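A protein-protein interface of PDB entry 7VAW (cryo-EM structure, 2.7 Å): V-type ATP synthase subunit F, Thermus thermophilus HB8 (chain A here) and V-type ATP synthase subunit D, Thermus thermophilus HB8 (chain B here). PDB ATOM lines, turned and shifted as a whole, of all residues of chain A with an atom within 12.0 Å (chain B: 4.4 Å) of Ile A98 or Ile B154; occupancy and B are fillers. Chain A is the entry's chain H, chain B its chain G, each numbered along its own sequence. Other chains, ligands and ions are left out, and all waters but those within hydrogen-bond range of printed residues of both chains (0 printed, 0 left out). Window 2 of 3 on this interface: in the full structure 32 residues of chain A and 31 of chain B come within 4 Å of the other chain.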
ATOM      1  N   GLU A  56      21.447  19.294  37.123  1.00  0.00           N
ATOM      2  CA  GLU A  56      21.102  18.841  35.783  1.00  0.00           C
ATOM      3  C   GLU A  56      21.030  17.323  35.696  1.00  0.00           C
ATOM      4  O   GLU A  56      20.361  16.795  34.801  1.00  0.00           O
ATOM      5  CB  GLU A  56      22.111  19.378  34.768  1.00  0.00           C
ATOM      6  CG  GLU A  56      23.560  19.181  35.172  1.00  0.00           C
ATOM      7  CD  GLU A  56      24.155  20.424  35.797  1.00  0.00           C
ATOM      8  OE1 GLU A  56      23.592  20.913  36.799  1.00  0.00           O
ATOM      9  OE2 GLU A  56      25.176  20.922  35.279  1.00  0.00           O
ATOM     10  N   TYR A  89      32.383  29.844  38.923  1.00  0.00           N
ATOM     11  CA  TYR A  89      31.106  29.341  38.432  1.00  0.00           C
ATOM     12  C   TYR A  89      30.823  29.838  37.020  1.00  0.00           C
ATOM     13  O   TYR A  89      30.327  29.083  36.179  1.00  0.00           O
ATOM     14  CB  TYR A  89      29.974  29.747  39.371  1.00  0.00           C
ATOM     15  CG  TYR A  89      28.618  29.390  38.818  1.00  0.00           C
ATOM     16  CD1 TYR A  89      28.174  28.077  38.815  1.00  0.00           C
ATOM     17  CD2 TYR A  89      27.794  30.363  38.272  1.00  0.00           C
ATOM     18  CE1 TYR A  89      26.938  27.743  38.299  1.00  0.00           C
ATOM     19  CE2 TYR A  89      26.562  30.040  37.753  1.00  0.00           C
ATOM     20  CZ  TYR A  89      26.135  28.729  37.770  1.00  0.00           C
ATOM     21  OH  TYR A  89      24.902  28.401  37.254  1.00  0.00           O
ATOM     22  N   MET A  90      31.122  31.108  36.742  1.00  0.00           N
ATOM     23  CA  MET A  90      30.899  31.630  35.398  1.00  0.00           C
ATOM     24  C   MET A  90      31.784  30.925  34.377  1.00  0.00           C
ATOM     25  O   MET A  90      31.333  30.591  33.275  1.00  0.00           O
ATOM     26  CB  MET A  90      31.140  33.138  35.377  1.00  0.00           C
ATOM     27  CG  MET A  90      30.204  33.904  34.461  1.00  0.00           C
ATOM     28  SD  MET A  90      28.458  33.686  34.859  1.00  0.00           S
ATOM     29  CE  MET A  90      28.463  33.911  36.637  1.00  0.00           C
ATOM     30  N   ARG A  91      33.051  30.693  34.727  1.00  0.00           N
ATOM     31  CA  ARG A  91      33.952  29.990  33.820  1.00  0.00           C
ATOM     32  C   ARG A  91      33.483  28.562  33.571  1.00  0.00           C
ATOM     33  O   ARG A  91      33.476  28.093  32.427  1.00  0.00           O
ATOM     34  CB  ARG A  91      35.373  29.998  34.378  1.00  0.00           C
ATOM     35  CG  ARG A  91      36.195  31.191  33.936  1.00  0.00           C
ATOM     36  CD  ARG A  91      37.604  31.149  34.499  1.00  0.00           C
ATOM     37  NE  ARG A  91      37.651  31.575  35.893  1.00  0.00           N
ATOM     38  CZ  ARG A  91      37.705  30.748  36.927  1.00  0.00           C
ATOM     39  NH1 ARG A  91      37.706  29.436  36.764  1.00  0.00           N
ATOM     40  NH2 ARG A  91      37.763  31.251  38.157  1.00  0.00           N
ATOM     41  N   GLU A  92      33.072  27.856  34.627  1.00  0.00           N
ATOM     42  CA  GLU A  92      32.600  26.493  34.426  1.00  0.00           C
ATOM     43  C   GLU A  92      31.300  26.472  33.634  1.00  0.00           C
ATOM     44  O   GLU A  92      31.078  25.549  32.848  1.00  0.00           O
ATOM     45  CB  GLU A  92      32.443  25.767  35.766  1.00  0.00           C
ATOM     46  CG  GLU A  92      31.257  26.191  36.615  1.00  0.00           C
ATOM     47  CD  GLU A  92      29.999  25.406  36.297  1.00  0.00           C
ATOM     48  OE1 GLU A  92      30.115  24.307  35.715  1.00  0.00           O
ATOM     49  OE2 GLU A  92      28.895  25.889  36.623  1.00  0.00           O
ATOM     50  N   LEU A  93      30.450  27.488  33.795  1.00  0.00           N
ATOM     51  CA  LEU A  93      29.205  27.548  33.036  1.00  0.00           C
ATOM     52  C   LEU A  93      29.471  27.786  31.554  1.00  0.00           C
ATOM     53  O   LEU A  93      28.888  27.113  30.692  1.00  0.00           O
ATOM     54  CB  LEU A  93      28.308  28.645  33.606  1.00  0.00           C
ATOM     55  CG  LEU A  93      27.015  28.961  32.854  1.00  0.00           C
ATOM     56  CD1 LEU A  93      26.152  27.722  32.710  1.00  0.00           C
ATOM     57  CD2 LEU A  93      26.259  30.060  33.576  1.00  0.00           C
ATOM     58  N   VAL A  94      30.347  28.742  31.237  1.00  0.00           N
ATOM     59  CA  VAL A  94      30.645  29.018  29.835  1.00  0.00           C
ATOM     60  C   VAL A  94      31.352  27.827  29.199  1.00  0.00           C
ATOM     61  O   VAL A  94      31.133  27.518  28.022  1.00  0.00           O
ATOM     62  CB  VAL A  94      31.453  30.324  29.688  1.00  0.00           C
ATOM     63  CG1 VAL A  94      32.830  30.199  30.301  1.00  0.00           C
ATOM     64  CG2 VAL A  94      31.560  30.720  28.225  1.00  0.00           C
ATOM     65  N   ARG A  95      32.195  27.128  29.962  1.00  0.00           N
ATOM     66  CA  ARG A  95      32.789  25.896  29.454  1.00  0.00           C
ATOM     67  C   ARG A  95      31.731  24.819  29.243  1.00  0.00           C
ATOM     68  O   ARG A  95      31.780  24.072  28.261  1.00  0.00           O
ATOM     69  CB  ARG A  95      33.872  25.411  30.416  1.00  0.00           C
ATOM     70  CG  ARG A  95      34.739  24.290  29.873  1.00  0.00           C
ATOM     71  CD  ARG A  95      35.693  23.792  30.944  1.00  0.00           C
ATOM     72  NE  ARG A  95      35.006  22.993  31.951  1.00  0.00           N
ATOM     73  CZ  ARG A  95      34.808  23.379  33.204  1.00  0.00           C
ATOM     74  NH1 ARG A  95      35.223  24.558  33.637  1.00  0.00           N
ATOM     75  NH2 ARG A  95      34.179  22.562  34.043  1.00  0.00           N
ATOM     76  N   LYS A  96      30.768  24.721  30.161  1.00  0.00           N
ATOM     77  CA  LYS A  96      29.745  23.687  30.067  1.00  0.00           C
ATOM     78  C   LYS A  96      28.859  23.892  28.848  1.00  0.00           C
ATOM     79  O   LYS A  96      28.476  22.925  28.180  1.00  0.00           O
ATOM     80  CB  LYS A  96      28.906  23.674  31.346  1.00  0.00           C
ATOM     81  CG  LYS A  96      27.894  22.544  31.421  1.00  0.00           C
ATOM     82  CD  LYS A  96      28.584  21.199  31.558  1.00  0.00           C
ATOM     83  CE  LYS A  96      27.575  20.084  31.769  1.00  0.00           C
ATOM     84  NZ  LYS A  96      26.954  19.656  30.486  1.00  0.00           N
ATOM     85  N   THR A  97      28.521  25.145  28.539  1.00  0.00           N
ATOM     86  CA  THR A  97      27.609  25.416  27.436  1.00  0.00           C
ATOM     87  C   THR A  97      28.310  25.732  26.120  1.00  0.00           C
ATOM     88  O   THR A  97      27.652  25.722  25.074  1.00  0.00           O
ATOM     89  CB  THR A  97      26.667  26.573  27.794  1.00  0.00           C
ATOM     90  OG1 THR A  97      25.651  26.692  26.791  1.00  0.00           O
ATOM     91  CG2 THR A  97      27.435  27.876  27.884  1.00  0.00           C
ATOM     92  N   ILE A  98      29.618  26.002  26.135  1.00  0.00           N
ATOM     93  CA  ILE A  98      30.389  26.259  24.922  1.00  0.00           C
ATOM     94  C   ILE A  98      31.563  25.295  24.791  1.00  0.00           C
ATOM     95  O   ILE A  98      31.686  24.583  23.788  1.00  0.00           O
ATOM     96  CB  ILE A  98      30.874  27.724  24.860  1.00  0.00           C
ATOM     97  CG1 ILE A  98      29.680  28.678  24.878  1.00  0.00           C
ATOM     98  CG2 ILE A  98      31.730  27.952  23.625  1.00  0.00           C
ATOM     99  CD1 ILE A  98      28.727  28.477  23.723  1.00  0.00           C
ATOM    100  N   GLY A  99      32.441  25.264  25.789  1.00  0.00           N
ATOM    101  CA  GLY A  99      33.545  24.327  25.782  1.00  0.00           C
ATOM    102  C   GLY A  99      34.802  24.794  25.086  1.00  0.00           C
ATOM    103  O   GLY A  99      35.368  24.039  24.287  1.00  0.00           O
ATOM    104  N   PHE A 100      35.263  26.017  25.360  1.00  0.00           N
ATOM    105  CA  PHE A 100      36.472  26.529  24.729  1.00  0.00           C
ATOM    106  C   PHE A 100      37.393  27.258  25.701  1.00  0.00           C
ATOM    107  O   PHE A 100      38.444  27.755  25.278  1.00  0.00           O
ATOM    108  CB  PHE A 100      36.116  27.451  23.559  1.00  0.00           C
ATOM    109  CG  PHE A 100      35.834  26.719  22.280  1.00  0.00           C
ATOM    110  CD1 PHE A 100      34.575  26.197  22.027  1.00  0.00           C
ATOM    111  CD2 PHE A 100      36.830  26.541  21.334  1.00  0.00           C
ATOM    112  CE1 PHE A 100      34.316  25.519  20.852  1.00  0.00           C
ATOM    113  CE2 PHE A 100      36.576  25.864  20.158  1.00  0.00           C
ATOM    114  CZ  PHE A 100      35.317  25.353  19.916  1.00  0.00           C
ATOM    115  N   ASP A 101      37.036  27.328  26.986  1.00  0.00           N
ATOM    116  CA  ASP A 101      37.886  27.933  28.015  1.00  0.00           C
ATOM    117  C   ASP A 101      38.271  29.367  27.656  1.00  0.00           C
ATOM    118  O   ASP A 101      39.426  29.773  27.795  1.00  0.00           O
ATOM    119  CB  ASP A 101      39.135  27.084  28.264  1.00  0.00           C
ATOM    120  CG  ASP A 101      38.804  25.641  28.575  1.00  0.00           C
ATOM    121  OD1 ASP A 101      37.649  25.368  28.961  1.00  0.00           O
ATOM    122  OD2 ASP A 101      39.695  24.778  28.433  1.00  0.00           O
ATOM    123  N   ILE A 102      37.295  30.139  27.187  1.00  0.00           N
ATOM    124  CA  ILE A 102      37.536  31.494  26.708  1.00  0.00           C
ATOM    125  C   ILE A 102      37.184  32.478  27.817  1.00  0.00           C
ATOM    126  O   ILE A 102      36.008  32.701  28.110  1.00  0.00           O
ATOM    127  CB  ILE A 102      36.731  31.786  25.436  1.00  0.00           C
ATOM    128  CG1 ILE A 102      37.127  30.817  24.321  1.00  0.00           C
ATOM    129  CG2 ILE A 102      36.933  33.224  25.005  1.00  0.00           C
ATOM    130  CD1 ILE A 102      38.612  30.789  24.038  1.00  0.00           C
ATOM    131  N   LYS A 103      38.209  33.080  28.420  1.00  0.00           N
ATOM    132  CA  LYS A 103      38.036  34.147  29.395  1.00  0.00           C
ATOM    133  C   LYS A 103      39.272  35.033  29.388  1.00  0.00           C
ATOM    134  O   LYS A 103      40.402  34.547  29.481  1.00  0.00           O
ATOM    135  CB  LYS A 103      37.794  33.610  30.813  1.00  0.00           C
ATOM    136  CG  LYS A 103      36.354  33.223  31.113  1.00  0.00           C
ATOM    137  CD  LYS A 103      35.399  34.389  30.898  1.00  0.00           C
ATOM    138  CE  LYS A 103      35.661  35.506  31.896  1.00  0.00           C
ATOM    139  NZ  LYS A 103      34.757  36.668  31.685  1.00  0.00           N
ATOM    140  N   LEU B  35      25.020  35.418  17.631  1.00  0.00           N
ATOM    141  CA  LEU B  35      24.685  34.659  18.829  1.00  0.00           C
ATOM    142  C   LEU B  35      25.803  34.732  19.860  1.00  0.00           C
ATOM    143  O   LEU B  35      25.540  34.822  21.061  1.00  0.00           O
ATOM    144  CB  LEU B  35      24.393  33.206  18.464  1.00  0.00           C
ATOM    145  CG  LEU B  35      23.028  32.906  17.850  1.00  0.00           C
ATOM    146  CD1 LEU B  35      23.044  31.552  17.170  1.00  0.00           C
ATOM    147  CD2 LEU B  35      21.943  32.965  18.907  1.00  0.00           C
ATOM    148  N   VAL B  36      27.057  34.683  19.409  1.00  0.00           N
ATOM    149  CA  VAL B  36      28.190  34.741  20.325  1.00  0.00           C
ATOM    150  C   VAL B  36      28.279  36.111  20.982  1.00  0.00           C
ATOM    151  O   VAL B  36      28.577  36.222  22.177  1.00  0.00           O
ATOM    152  CB  VAL B  36      29.490  34.375  19.586  1.00  0.00           C
ATOM    153  CG1 VAL B  36      30.705  34.793  20.393  1.00  0.00           C
ATOM    154  CG2 VAL B  36      29.535  32.885  19.315  1.00  0.00           C
ATOM    155  N   PHE B  39      25.613  36.152  23.568  1.00  0.00           N
ATOM    156  CA  PHE B  39      25.981  35.253  24.654  1.00  0.00           C
ATOM    157  C   PHE B  39      27.024  35.881  25.565  1.00  0.00           C
ATOM    158  O   PHE B  39      26.958  35.734  26.790  1.00  0.00           O
ATOM    159  CB  PHE B  39      26.491  33.937  24.068  1.00  0.00           C
ATOM    160  CG  PHE B  39      27.029  32.974  25.084  1.00  0.00           C
ATOM    161  CD1 PHE B  39      28.371  32.980  25.420  1.00  0.00           C
ATOM    162  CD2 PHE B  39      26.200  32.045  25.681  1.00  0.00           C
ATOM    163  CE1 PHE B  39      28.870  32.093  26.345  1.00  0.00           C
ATOM    164  CE2 PHE B  39      26.695  31.153  26.608  1.00  0.00           C
ATOM    165  CZ  PHE B  39      28.032  31.178  26.939  1.00  0.00           C
ATOM    166  N   ILE B 150      20.603  30.591  24.831  1.00  0.00           N
ATOM    167  CA  ILE B 150      21.494  31.140  23.811  1.00  0.00           C
ATOM    168  C   ILE B 150      22.648  30.182  23.537  1.00  0.00           C
ATOM    169  O   ILE B 150      23.069  30.009  22.387  1.00  0.00           O
ATOM    170  CB  ILE B 150      21.996  32.536  24.223  1.00  0.00           C
ATOM    171  CG1 ILE B 150      20.820  33.497  24.389  1.00  0.00           C
ATOM    172  CG2 ILE B 150      22.957  33.082  23.189  1.00  0.00           C
ATOM    173  CD1 ILE B 150      19.866  33.507  23.218  1.00  0.00           C
ATOM    174  N   GLY B 151      23.174  29.538  24.579  1.00  0.00           N
ATOM    175  CA  GLY B 151      24.234  28.564  24.371  1.00  0.00           C
ATOM    176  C   GLY B 151      23.768  27.353  23.585  1.00  0.00           C
ATOM    177  O   GLY B 151      24.500  26.824  22.745  1.00  0.00           O
ATOM    178  N   GLU B 152      22.542  26.899  23.845  1.00  0.00           N
ATOM    179  CA  GLU B 152      21.990  25.794  23.069  1.00  0.00           C
ATOM    180  C   GLU B 152      21.802  26.191  21.611  1.00  0.00           C
ATOM    181  O   GLU B 152      22.048  25.390  20.705  1.00  0.00           O
ATOM    182  CB  GLU B 152      20.667  25.331  23.678  1.00  0.00           C
ATOM    183  CG  GLU B 152      20.077  24.105  23.003  1.00  0.00           C
ATOM    184  CD  GLU B 152      18.912  23.515  23.773  1.00  0.00           C
ATOM    185  OE1 GLU B 152      18.074  24.292  24.277  1.00  0.00           O
ATOM    186  OE2 GLU B 152      18.831  22.272  23.870  1.00  0.00           O
ATOM    187  N   GLU B 153      21.365  27.428  21.366  1.00  0.00           N
ATOM    188  CA  GLU B 153      21.235  27.907  19.994  1.00  0.00           C
ATOM    189  C   GLU B 153      22.591  27.973  19.303  1.00  0.00           C
ATOM    190  O   GLU B 153      22.713  27.639  18.116  1.00  0.00           O
ATOM    191  CB  GLU B 153      20.551  29.273  19.979  1.00  0.00           C
ATOM    192  CG  GLU B 153      20.139  29.752  18.600  1.00  0.00           C
ATOM    193  CD  GLU B 153      19.062  28.892  17.969  1.00  0.00           C
ATOM    194  OE1 GLU B 153      18.271  28.277  18.715  1.00  0.00           O
ATOM    195  OE2 GLU B 153      19.006  28.831  16.724  1.00  0.00           O
ATOM    196  N   ILE B 154      23.627  28.404  20.028  1.00  0.00           N
ATOM    197  CA  ILE B 154      24.974  28.418  19.464  1.00  0.00           C
ATOM    198  C   ILE B 154      25.414  27.006  19.113  1.00  0.00           C
ATOM    199  O   ILE B 154      26.003  26.767  18.053  1.00  0.00           O
ATOM    200  CB  ILE B 154      25.963  29.090  20.434  1.00  0.00           C
ATOM    201  CG1 ILE B 154      25.713  30.592  20.496  1.00  0.00           C
ATOM    202  CG2 ILE B 154      27.396  28.823  20.007  1.00  0.00           C
ATOM    203  CD1 ILE B 154      26.422  31.268  21.631  1.00  0.00           C
ATOM    204  N   LYS B 155      25.144  26.048  20.001  1.00  0.00           N
ATOM    205  CA  LYS B 155      25.515  24.664  19.724  1.00  0.00           C
ATOM    206  C   LYS B 155      24.763  24.120  18.515  1.00  0.00           C
ATOM    207  O   LYS B 155      25.326  23.375  17.709  1.00  0.00           O
ATOM    208  CB  LYS B 155      25.265  23.796  20.956  1.00  0.00           C
ATOM    209  CG  LYS B 155      26.293  23.998  22.057  1.00  0.00           C
ATOM    210  CD  LYS B 155      25.901  23.271  23.330  1.00  0.00           C
ATOM    211  CE  LYS B 155      25.854  21.770  23.114  1.00  0.00           C
ATOM    212  NZ  LYS B 155      25.567  21.038  24.377  1.00  0.00           N
ATOM    213  N   LYS B 156      23.487  24.481  18.375  1.00  0.00           N
ATOM    214  CA  LYS B 156      22.707  24.042  17.221  1.00  0.00           C
ATOM    215  C   LYS B 156      23.268  24.614  15.924  1.00  0.00           C
ATOM    216  O   LYS B 156      23.399  23.898  14.920  1.00  0.00           O
ATOM    217  CB  LYS B 156      21.246  24.454  17.400  1.00  0.00           C
ATOM    218  CG  LYS B 156      20.266  23.704  16.522  1.00  0.00           C
ATOM    219  CD  LYS B 156      20.176  22.243  16.926  1.00  0.00           C
ATOM    220  CE  LYS B 156      18.883  21.614  16.433  1.00  0.00           C
ATOM    221  NZ  LYS B 156      18.814  21.579  14.947  1.00  0.00           N
ATOM    222  N   THR B 157      23.605  25.906  15.927  1.00  0.00           N
ATOM    223  CA  THR B 157      24.202  26.517  14.743  1.00  0.00           C
ATOM    224  C   THR B 157      25.548  25.882  14.417  1.00  0.00           C
ATOM    225  O   THR B 157      25.868  25.662  13.244  1.00  0.00           O
ATOM    226  CB  THR B 157      24.352  28.023  14.945  1.00  0.00           C
ATOM    227  OG1 THR B 157      23.060  28.611  15.131  1.00  0.00           O
ATOM    228  CG2 THR B 157      25.021  28.658  13.741  1.00  0.00           C
ATOM    229  N   THR B 158      26.349  25.585  15.440  1.00  0.00           N
ATOM    230  CA  THR B 158      27.623  24.911  15.214  1.00  0.00           C
ATOM    231  C   THR B 158      27.412  23.525  14.621  1.00  0.00           C
ATOM    232  O   THR B 158      28.147  23.115  13.717  1.00  0.00           O
ATOM    233  CB  THR B 158      28.405  24.819  16.522  1.00  0.00           C
ATOM    234  OG1 THR B 158      28.658  26.137  17.021  1.00  0.00           O
ATOM    235  CG2 THR B 158      29.728  24.112  16.302  1.00  0.00           C
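OG1 of Thr B158 sits at hydrogen-bond distance from O of Ile B154 (2.9 Å).
The backbone NH (N) of Gly A99 sits at hydrogen-bond distance from the backbone carbonyl oxygen (O) of Val A94 (3.4 Å).
Among the printed residues, merely in contact across the chains: Val A94 with Phe B39, Thr A97 with Phe B39, Thr A97 with Gly B151, Thr A97 with Lys B155, Ile A98 with Phe B39 and Ile A98 with Ile B154.
Printed residues of chain B within 4 Å of Val A94: Phe B39 (3.6 Å).
Of the printed residues of chain B, Thr A97 touches Phe B39, Gly B151 and Lys B155.
Of chain B, only Phe B39 (3.6 Å) and Ile B154 (3.96 Å) come within 4 Å of Ile A98.
No residue of chain A comes within 4 Å of Leu B35.
No residue of chain A comes within 4 Å of Glu B153.
Ile B154 touches just one residue of chain A: Ile A98.
Lys B155 touches just one residue of chain A: Thr A97.
No residue of chain A comes within 4 Å of Thr B157.
The nearest printed residue of chain B that does not touch Ile A98 is Gly B151 (4.5 Å).
Of the 12 printed residues of chain B, 4 touch a printed residue of chain A.
Hydrophobic or aromatic side chains of chain B that line the printed part of chain A: Phe B39 and Ile B154.
Along chain B the printed residues that touch a printed residue of chain A span positions 39 to 155.
Among the printed residues, 6 pairs touch across the chains.
Among the printed residues, no Asp or Glu carboxylate lies within 4 Å of a Lys or Arg side-chain nitrogen of the other chain.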
